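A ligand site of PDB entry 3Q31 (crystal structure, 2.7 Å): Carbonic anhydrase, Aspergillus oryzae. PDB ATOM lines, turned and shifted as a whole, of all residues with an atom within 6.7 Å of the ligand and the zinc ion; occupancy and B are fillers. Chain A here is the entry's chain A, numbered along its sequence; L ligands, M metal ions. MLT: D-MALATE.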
ATOM      1  N   PHE A  11      15.034 -11.792 -19.829  1.00  0.00           N
ATOM      2  CA  PHE A  11      15.164 -11.086 -18.570  1.00  0.00           C
ATOM      3  C   PHE A  11      16.053 -11.880 -17.584  1.00  0.00           C
ATOM      4  O   PHE A  11      15.559 -12.525 -16.656  1.00  0.00           O
ATOM      5  CB  PHE A  11      13.786 -10.752 -17.987  1.00  0.00           C
ATOM      6  CG  PHE A  11      13.830 -10.112 -16.615  1.00  0.00           C
ATOM      7  CD1 PHE A  11      12.718 -10.110 -15.807  1.00  0.00           C
ATOM      8  CD2 PHE A  11      14.992  -9.535 -16.145  1.00  0.00           C
ATOM      9  CE1 PHE A  11      12.758  -9.546 -14.557  1.00  0.00           C
ATOM     10  CE2 PHE A  11      15.023  -8.985 -14.882  1.00  0.00           C
ATOM     11  CZ  PHE A  11      13.911  -8.991 -14.095  1.00  0.00           C
ATOM     12  N   TYR A  13      20.361 -11.970 -15.776  1.00  0.00           N
ATOM     13  CA  TYR A  13      21.407 -11.179 -15.104  1.00  0.00           C
ATOM     14  C   TYR A  13      22.758 -11.422 -15.748  1.00  0.00           C
ATOM     15  O   TYR A  13      23.753 -10.754 -15.474  1.00  0.00           O
ATOM     16  CB  TYR A  13      21.459 -11.470 -13.603  1.00  0.00           C
ATOM     17  CG  TYR A  13      20.338 -10.795 -12.844  1.00  0.00           C
ATOM     18  CD1 TYR A  13      20.475  -9.497 -12.371  1.00  0.00           C
ATOM     19  CD2 TYR A  13      19.142 -11.453 -12.616  1.00  0.00           C
ATOM     20  CE1 TYR A  13      19.447  -8.870 -11.698  1.00  0.00           C
ATOM     21  CE2 TYR A  13      18.115 -10.840 -11.943  1.00  0.00           C
ATOM     22  CZ  TYR A  13      18.264  -9.556 -11.484  1.00  0.00           C
ATOM     23  OH  TYR A  13      17.219  -8.965 -10.804  1.00  0.00           O
ATOM     24  N   LEU A  71      11.102 -17.979  -9.191  1.00  0.00           N
ATOM     25  CA  LEU A  71      11.062 -17.148 -10.389  1.00  0.00           C
ATOM     26  C   LEU A  71      12.062 -17.541 -11.468  1.00  0.00           C
ATOM     27  O   LEU A  71      11.897 -17.195 -12.627  1.00  0.00           O
ATOM     28  CB  LEU A  71      11.338 -15.689 -10.019  1.00  0.00           C
ATOM     29  CG  LEU A  71      10.263 -14.961  -9.223  1.00  0.00           C
ATOM     30  CD1 LEU A  71      10.648 -13.488  -9.164  1.00  0.00           C
ATOM     31  CD2 LEU A  71       8.904 -15.166  -9.869  1.00  0.00           C
ATOM     32  N   GLN A  76      10.084 -15.385  -4.691  1.00  0.00           N
ATOM     33  CA  GLN A  76       9.013 -14.440  -4.393  1.00  0.00           C
ATOM     34  C   GLN A  76       7.817 -15.081  -3.697  1.00  0.00           C
ATOM     35  O   GLN A  76       7.323 -16.165  -4.066  1.00  0.00           O
ATOM     36  CB  GLN A  76       8.555 -13.786  -5.687  1.00  0.00           C
ATOM     37  CG  GLN A  76       7.470 -12.783  -5.514  1.00  0.00           C
ATOM     38  CD  GLN A  76       7.220 -11.965  -6.769  1.00  0.00           C
ATOM     39  OE1 GLN A  76       8.102 -11.826  -7.617  1.00  0.00           O
ATOM     40  NE2 GLN A  76       6.008 -11.433  -6.890  1.00  0.00           N
ATOM     41  N   GLN A  95       3.399  -8.319  -3.204  1.00  0.00           N
ATOM     42  CA  GLN A  95       4.323  -9.455  -3.025  1.00  0.00           C
ATOM     43  C   GLN A  95       5.614  -9.007  -2.353  1.00  0.00           C
ATOM     44  O   GLN A  95       5.950  -7.820  -2.356  1.00  0.00           O
ATOM     45  CB  GLN A  95       4.669 -10.095  -4.369  1.00  0.00           C
ATOM     46  CG  GLN A  95       5.047  -9.086  -5.487  1.00  0.00           C
ATOM     47  CD  GLN A  95       6.537  -8.751  -5.553  1.00  0.00           C
ATOM     48  OE1 GLN A  95       7.379  -9.433  -4.968  1.00  0.00           O
ATOM     49  NE2 GLN A  95       6.871  -7.690  -6.281  1.00  0.00           N
ATOM     50  N   HIS A  97       9.974 -10.237  -2.084  1.00  0.00           N
ATOM     51  CA  HIS A  97      10.961 -11.131  -2.685  1.00  0.00           C
ATOM     52  C   HIS A  97      12.401 -10.802  -2.277  1.00  0.00           C
ATOM     53  O   HIS A  97      12.680  -9.805  -1.577  1.00  0.00           O
ATOM     54  CB  HIS A  97      10.818 -11.109  -4.197  1.00  0.00           C
ATOM     55  CG  HIS A  97      11.184  -9.793  -4.806  1.00  0.00           C
ATOM     56  ND1 HIS A  97      10.363  -8.691  -4.724  1.00  0.00           N
ATOM     57  CD2 HIS A  97      12.288  -9.394  -5.472  1.00  0.00           C
ATOM     58  CE1 HIS A  97      10.940  -7.665  -5.333  1.00  0.00           C
ATOM     59  NE2 HIS A  97      12.112  -8.066  -5.796  1.00  0.00           N
ATOM     60  N   PHE A  98      13.324 -11.648  -2.721  1.00  0.00           N
ATOM     61  CA  PHE A  98      14.674 -11.590  -2.213  1.00  0.00           C
ATOM     62  C   PHE A  98      15.693 -11.415  -3.294  1.00  0.00           C
ATOM     63  O   PHE A  98      15.517 -11.893  -4.414  1.00  0.00           O
ATOM     64  CB  PHE A  98      14.974 -12.834  -1.406  1.00  0.00           C
ATOM     65  CG  PHE A  98      13.988 -13.063  -0.327  1.00  0.00           C
ATOM     66  CD1 PHE A  98      12.791 -13.697  -0.607  1.00  0.00           C
ATOM     67  CD2 PHE A  98      14.226 -12.598   0.948  1.00  0.00           C
ATOM     68  CE1 PHE A  98      11.873 -13.890   0.373  1.00  0.00           C
ATOM     69  CE2 PHE A  98      13.288 -12.801   1.936  1.00  0.00           C
ATOM     70  CZ  PHE A  98      12.111 -13.433   1.642  1.00  0.00           C
ATOM     71  N   HIS A  99      16.755 -10.708  -2.941  1.00  0.00           N
ATOM     72  CA  HIS A  99      17.916 -10.535  -3.788  1.00  0.00           C
ATOM     73  C   HIS A  99      19.159 -10.951  -3.028  1.00  0.00           C
ATOM     74  O   HIS A  99      19.320 -10.682  -1.821  1.00  0.00           O
ATOM     75  CB  HIS A  99      18.081  -9.076  -4.146  1.00  0.00           C
ATOM     76  CG  HIS A  99      17.009  -8.538  -5.038  1.00  0.00           C
ATOM     77  ND1 HIS A  99      17.058  -8.668  -6.406  1.00  0.00           N
ATOM     78  CD2 HIS A  99      15.895  -7.830  -4.752  1.00  0.00           C
ATOM     79  CE1 HIS A  99      16.002  -8.066  -6.928  1.00  0.00           C
ATOM     80  NE2 HIS A  99      15.284  -7.565  -5.947  1.00  0.00           N
ATOM     81  N   GLU A 103      21.109  -5.330  -3.307  1.00  0.00           N
ATOM     82  CA  GLU A 103      21.210  -4.509  -4.499  1.00  0.00           C
ATOM     83  C   GLU A 103      21.734  -3.154  -4.096  1.00  0.00           C
ATOM     84  O   GLU A 103      22.638  -2.621  -4.737  1.00  0.00           O
ATOM     85  CB  GLU A 103      19.868  -4.392  -5.201  1.00  0.00           C
ATOM     86  CG  GLU A 103      19.262  -5.725  -5.618  1.00  0.00           C
ATOM     87  CD  GLU A 103      18.340  -5.589  -6.794  1.00  0.00           C
ATOM     88  OE1 GLU A 103      17.128  -5.326  -6.588  1.00  0.00           O
ATOM     89  OE2 GLU A 103      18.821  -5.728  -7.930  1.00  0.00           O
ATOM     90  N   GLU A 114      18.966  -8.955   0.424  1.00  0.00           N
ATOM     91  CA  GLU A 114      17.995  -7.872   0.541  1.00  0.00           C
ATOM     92  C   GLU A 114      16.578  -8.379   0.278  1.00  0.00           C
ATOM     93  O   GLU A 114      16.381  -9.124  -0.685  1.00  0.00           O
ATOM     94  CB  GLU A 114      18.366  -6.760  -0.440  1.00  0.00           C
ATOM     95  CG  GLU A 114      17.621  -5.463  -0.248  1.00  0.00           C
ATOM     96  CD  GLU A 114      18.220  -4.325  -1.059  1.00  0.00           C
ATOM     97  OE1 GLU A 114      19.435  -4.344  -1.373  1.00  0.00           O
ATOM     98  OE2 GLU A 114      17.470  -3.372  -1.370  1.00  0.00           O
ATOM     99  N   VAL A 115      15.599  -8.000   1.123  1.00  0.00           N
ATOM    100  CA  VAL A 115      14.162  -8.233   0.845  1.00  0.00           C
ATOM    101  C   VAL A 115      13.430  -6.992   0.371  1.00  0.00           C
ATOM    102  O   VAL A 115      13.622  -5.890   0.896  1.00  0.00           O
ATOM    103  CB  VAL A 115      13.327  -8.617   2.069  1.00  0.00           C
ATOM    104  CG1 VAL A 115      12.517  -9.897   1.795  1.00  0.00           C
ATOM    105  CG2 VAL A 115      14.166  -8.697   3.310  1.00  0.00           C
ATOM    106  N   HIS A 116      12.533  -7.213  -0.587  1.00  0.00           N
ATOM    107  CA  HIS A 116      11.724  -6.146  -1.136  1.00  0.00           C
ATOM    108  C   HIS A 116      10.251  -6.434  -0.920  1.00  0.00           C
ATOM    109  O   HIS A 116       9.734  -7.462  -1.387  1.00  0.00           O
ATOM    110  CB  HIS A 116      11.994  -6.002  -2.625  1.00  0.00           C
ATOM    111  CG  HIS A 116      13.333  -5.382  -2.919  1.00  0.00           C
ATOM    112  ND1 HIS A 116      13.975  -5.536  -4.140  1.00  0.00           N
ATOM    113  CD2 HIS A 116      14.139  -4.602  -2.168  1.00  0.00           C
ATOM    114  CE1 HIS A 116      15.121  -4.872  -4.113  1.00  0.00           C
ATOM    115  NE2 HIS A 116      15.240  -4.301  -2.934  1.00  0.00           N
ATOM    116  N   PHE A 117       9.577  -5.563  -0.178  1.00  0.00           N
ATOM    117  CA  PHE A 117       8.130  -5.656  -0.065  1.00  0.00           C
ATOM    118  C   PHE A 117       7.574  -4.626  -1.017  1.00  0.00           C
ATOM    119  O   PHE A 117       7.868  -3.423  -0.886  1.00  0.00           O
ATOM    120  CB  PHE A 117       7.667  -5.344   1.350  1.00  0.00           C
ATOM    121  CG  PHE A 117       7.918  -6.454   2.330  1.00  0.00           C
ATOM    122  CD1 PHE A 117       9.095  -6.505   3.056  1.00  0.00           C
ATOM    123  CD2 PHE A 117       6.977  -7.454   2.516  1.00  0.00           C
ATOM    124  CE1 PHE A 117       9.319  -7.530   3.967  1.00  0.00           C
ATOM    125  CE2 PHE A 117       7.193  -8.487   3.420  1.00  0.00           C
ATOM    126  CZ  PHE A 117       8.368  -8.524   4.145  1.00  0.00           C
ATOM    127  N   VAL A 118       6.806  -5.093  -1.995  1.00  0.00           N
ATOM    128  CA  VAL A 118       6.301  -4.220  -3.043  1.00  0.00           C
ATOM    129  C   VAL A 118       4.823  -3.877  -2.863  1.00  0.00           C
ATOM    130  O   VAL A 118       3.965  -4.769  -2.817  1.00  0.00           O
ATOM    131  CB  VAL A 118       6.496  -4.842  -4.429  1.00  0.00           C
ATOM    132  CG1 VAL A 118       6.132  -3.839  -5.482  1.00  0.00           C
ATOM    133  CG2 VAL A 118       7.921  -5.282  -4.604  1.00  0.00           C
ATOM    134  N   THR A 126       3.987   3.097  -7.118  1.00  0.00           N
ATOM    135  CA  THR A 126       4.634   2.049  -6.321  1.00  0.00           C
ATOM    136  C   THR A 126       5.458   2.594  -5.165  1.00  0.00           C
ATOM    137  O   THR A 126       6.010   3.699  -5.241  1.00  0.00           O
ATOM    138  CB  THR A 126       5.586   1.221  -7.168  1.00  0.00           C
ATOM    139  OG1 THR A 126       4.875   0.655  -8.282  1.00  0.00           O
ATOM    140  CG2 THR A 126       6.227   0.121  -6.309  1.00  0.00           C
ATOM    141  N   ALA A 127       5.545   1.811  -4.093  1.00  0.00           N
ATOM    142  CA  ALA A 127       6.448   2.086  -2.978  1.00  0.00           C
ATOM    143  C   ALA A 127       7.054   0.766  -2.548  1.00  0.00           C
ATOM    144  O   ALA A 127       6.418  -0.284  -2.669  1.00  0.00           O
ATOM    145  CB  ALA A 127       5.710   2.724  -1.810  1.00  0.00           C
ATOM    146  N   VAL A 128       8.295   0.802  -2.041  1.00  0.00           N
ATOM    147  CA  VAL A 128       8.924  -0.404  -1.537  1.00  0.00           C
ATOM    148  C   VAL A 128       9.356  -0.270  -0.085  1.00  0.00           C
ATOM    149  O   VAL A 128       9.810   0.795   0.368  1.00  0.00           O
ATOM    150  CB  VAL A 128      10.174  -0.786  -2.347  1.00  0.00           C
ATOM    151  CG1 VAL A 128      10.787  -2.045  -1.767  1.00  0.00           C
ATOM    152  CG2 VAL A 128       9.857  -0.976  -3.807  1.00  0.00           C
ATOM    153  N   SER A 187      13.579   3.823  -8.662  1.00  0.00           N
ATOM    154  CA  SER A 187      12.955   3.021  -9.697  1.00  0.00           C
ATOM    155  C   SER A 187      12.851   1.551  -9.311  1.00  0.00           C
ATOM    156  O   SER A 187      13.292   1.141  -8.238  1.00  0.00           O
ATOM    157  CB  SER A 187      13.782   3.094 -10.970  1.00  0.00           C
ATOM    158  OG  SER A 187      14.758   2.071 -10.937  1.00  0.00           O
ATOM    159  N   LEU A 188      12.265   0.777 -10.217  1.00  0.00           N
ATOM    160  CA  LEU A 188      12.248  -0.667 -10.100  1.00  0.00           C
ATOM    161  C   LEU A 188      13.628  -1.169 -10.439  1.00  0.00           C
ATOM    162  O   LEU A 188      14.280  -0.614 -11.326  1.00  0.00           O
ATOM    163  CB  LEU A 188      11.298  -1.252 -11.129  1.00  0.00           C
ATOM    164  CG  LEU A 188       9.828  -0.886 -10.970  1.00  0.00           C
ATOM    165  CD1 LEU A 188       8.996  -1.864 -11.810  1.00  0.00           C
ATOM    166  CD2 LEU A 188       9.462  -0.959  -9.500  1.00  0.00           C
ATOM    167  N   THR A 189      14.074  -2.209  -9.762  1.00  0.00           N
ATOM    168  CA  THR A 189      15.397  -2.752 -10.038  1.00  0.00           C
ATOM    169  C   THR A 189      15.307  -3.871 -11.066  1.00  0.00           C
ATOM    170  O   THR A 189      16.262  -4.598 -11.303  1.00  0.00           O
ATOM    171  CB  THR A 189      16.084  -3.233  -8.783  1.00  0.00           C
ATOM    172  OG1 THR A 189      15.308  -4.288  -8.189  1.00  0.00           O
ATOM    173  CG2 THR A 189      16.191  -2.084  -7.797  1.00  0.00           C
ATOM    174  N   THR A 190      14.132  -3.992 -11.682  1.00  0.00           N
ATOM    175  CA  THR A 190      13.940  -4.940 -12.756  1.00  0.00           C
ATOM    176  C   THR A 190      13.206  -4.224 -13.877  1.00  0.00           C
ATOM    177  O   THR A 190      12.590  -3.189 -13.649  1.00  0.00           O
ATOM    178  CB  THR A 190      13.159  -6.212 -12.301  1.00  0.00           C
ATOM    179  OG1 THR A 190      12.011  -5.850 -11.534  1.00  0.00           O
ATOM    180  CG2 THR A 190      14.045  -7.088 -11.444  1.00  0.00           C
ATOM    181  N   PRO A 191      13.285  -4.767 -15.085  1.00  0.00           N
ATOM    182  CA  PRO A 191      12.626  -4.123 -16.229  1.00  0.00           C
ATOM    183  C   PRO A 191      11.119  -4.067 -15.985  1.00  0.00           C
ATOM    184  O   PRO A 191      10.528  -5.048 -15.517  1.00  0.00           O
ATOM    185  CB  PRO A 191      12.935  -5.075 -17.389  1.00  0.00           C
ATOM    186  CG  PRO A 191      14.072  -5.954 -16.901  1.00  0.00           C
ATOM    187  CD  PRO A 191      13.860  -6.065 -15.439  1.00  0.00           C
ATOM    188  N   VAL A 197       9.460   5.334  -7.992  1.00  0.00           N
ATOM    189  CA  VAL A 197       9.238   4.387  -6.909  1.00  0.00           C
ATOM    190  C   VAL A 197       9.624   5.010  -5.581  1.00  0.00           C
ATOM    191  O   VAL A 197      10.627   5.704  -5.483  1.00  0.00           O
ATOM    192  CB  VAL A 197      10.062   3.110  -7.086  1.00  0.00           C
ATOM    193  CG1 VAL A 197       9.936   2.216  -5.839  1.00  0.00           C
ATOM    194  CG2 VAL A 197       9.623   2.375  -8.367  1.00  0.00           C
ATOM    195  N   TRP A 199      11.169   4.596  -2.268  1.00  0.00           N
ATOM    196  CA  TRP A 199      12.040   3.651  -1.611  1.00  0.00           C
ATOM    197  C   TRP A 199      12.142   3.910  -0.121  1.00  0.00           C
ATOM    198  O   TRP A 199      12.442   5.028   0.327  1.00  0.00           O
ATOM    199  CB  TRP A 199      13.424   3.638  -2.279  1.00  0.00           C
ATOM    200  CG  TRP A 199      13.491   2.711  -3.438  1.00  0.00           C
ATOM    201  CD1 TRP A 199      13.318   3.018  -4.753  1.00  0.00           C
ATOM    202  CD2 TRP A 199      13.743   1.302  -3.377  1.00  0.00           C
ATOM    203  NE1 TRP A 199      13.459   1.889  -5.535  1.00  0.00           N
ATOM    204  CE2 TRP A 199      13.717   0.819  -4.717  1.00  0.00           C
ATOM    205  CE3 TRP A 199      14.008   0.405  -2.336  1.00  0.00           C
ATOM    206  CZ2 TRP A 199      13.924  -0.521  -5.029  1.00  0.00           C
ATOM    207  CZ3 TRP A 199      14.216  -0.941  -2.655  1.00  0.00           C
ATOM    208  CH2 TRP A 199      14.167  -1.384  -3.994  1.00  0.00           C
HETATM  209  C1  MLT L   1      10.174  -6.090  -8.869  1.00  0.00           C
HETATM  210  O1  MLT L   1       9.522  -7.055  -8.422  1.00  0.00           O
HETATM  211  O2  MLT L   1       9.740  -5.497  -9.881  1.00  0.00           O
HETATM  212  C2  MLT L   1      11.444  -5.623  -8.190  1.00  0.00           C
HETATM  213  O3  MLT L   1      12.655  -6.148  -8.727  1.00  0.00           O
HETATM  214  C3  MLT L   1      11.556  -4.123  -8.009  1.00  0.00           C
HETATM  215  C4  MLT L   1      11.742  -4.050  -6.530  1.00  0.00           C
HETATM  216  O4  MLT L   1      11.584  -2.975  -5.905  1.00  0.00           O
HETATM  217  O5  MLT L   1      12.029  -5.113  -5.909  1.00  0.00           O
HETATM  218 ZN    ZN M   1      13.474  -6.512  -5.928  1.00  0.00          ZN
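Glu 103 touches the zinc ion. Thr 189 touches the zinc ion. Within 4 Å of the zinc ion: His 97, His 99, Glu 103, His 116 and Thr 189.
O2 of the ligand is in hydrogen-bond range of OG1 of Thr 190. The side-chain hydroxyl (OG1) of Thr 189 is in hydrogen-bond range of an oxygen (O3) of the ligand (3.3 Å). The side-chain amide nitrogen (NE2) of Gln 95 is in hydrogen-bond range of an oxygen (O1) of the ligand (3.5 Å).
OE1 of Glu 114 is in hydrogen-bond range of N of Glu 103 (2.7 Å). OE2 of Glu 114 lies within hydrogen-bond range of NE2 of His 116 (2.9 Å). O of Glu 114 is in hydrogen-bond range of N of His 99, at 2.8 Å. A ring nitrogen (ND1) of His 97 sits at hydrogen-bond distance from the side-chain amide oxygen (OE1) of Gln 95. The side-chain amide oxygen (OE1) of Gln 95 lies close to the side-chain amide nitrogen (NE2) of Gln 76 (3.1 Å). The backbone carbonyl oxygen (O) of Ser 187 lies within hydrogen-bond range of the indole nitrogen (NE1) of Trp 199. OG1 of Thr 189 lies within hydrogen-bond range of OE1 of Glu 103. The side-chain carboxylate (OE1) of Glu 103 sits close to a ring nitrogen (ND1) of His 99.
O5 of the ligand binds the zinc ion. NE2 of His 97 binds the zinc ion (2.1 Å). NE2 of His 99 binds the zinc ion. The zinc ion is bound by ND1 of His 116 (2.1 Å). The zinc ion has four donor atoms within binding distance.
Val 128 touches the ligand (CG2 to O4, 3.4 Å). Trp 199 touches the ligand. Hydrophobic or aromatic side chains that line the ligand: His 97, His 116, Val 128 and Trp 199. Of the 24 residues printed, 7 come within 4 Å of the ligand. Along chain A the residues within 4 Å of the ligand span positions 95 to 199.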
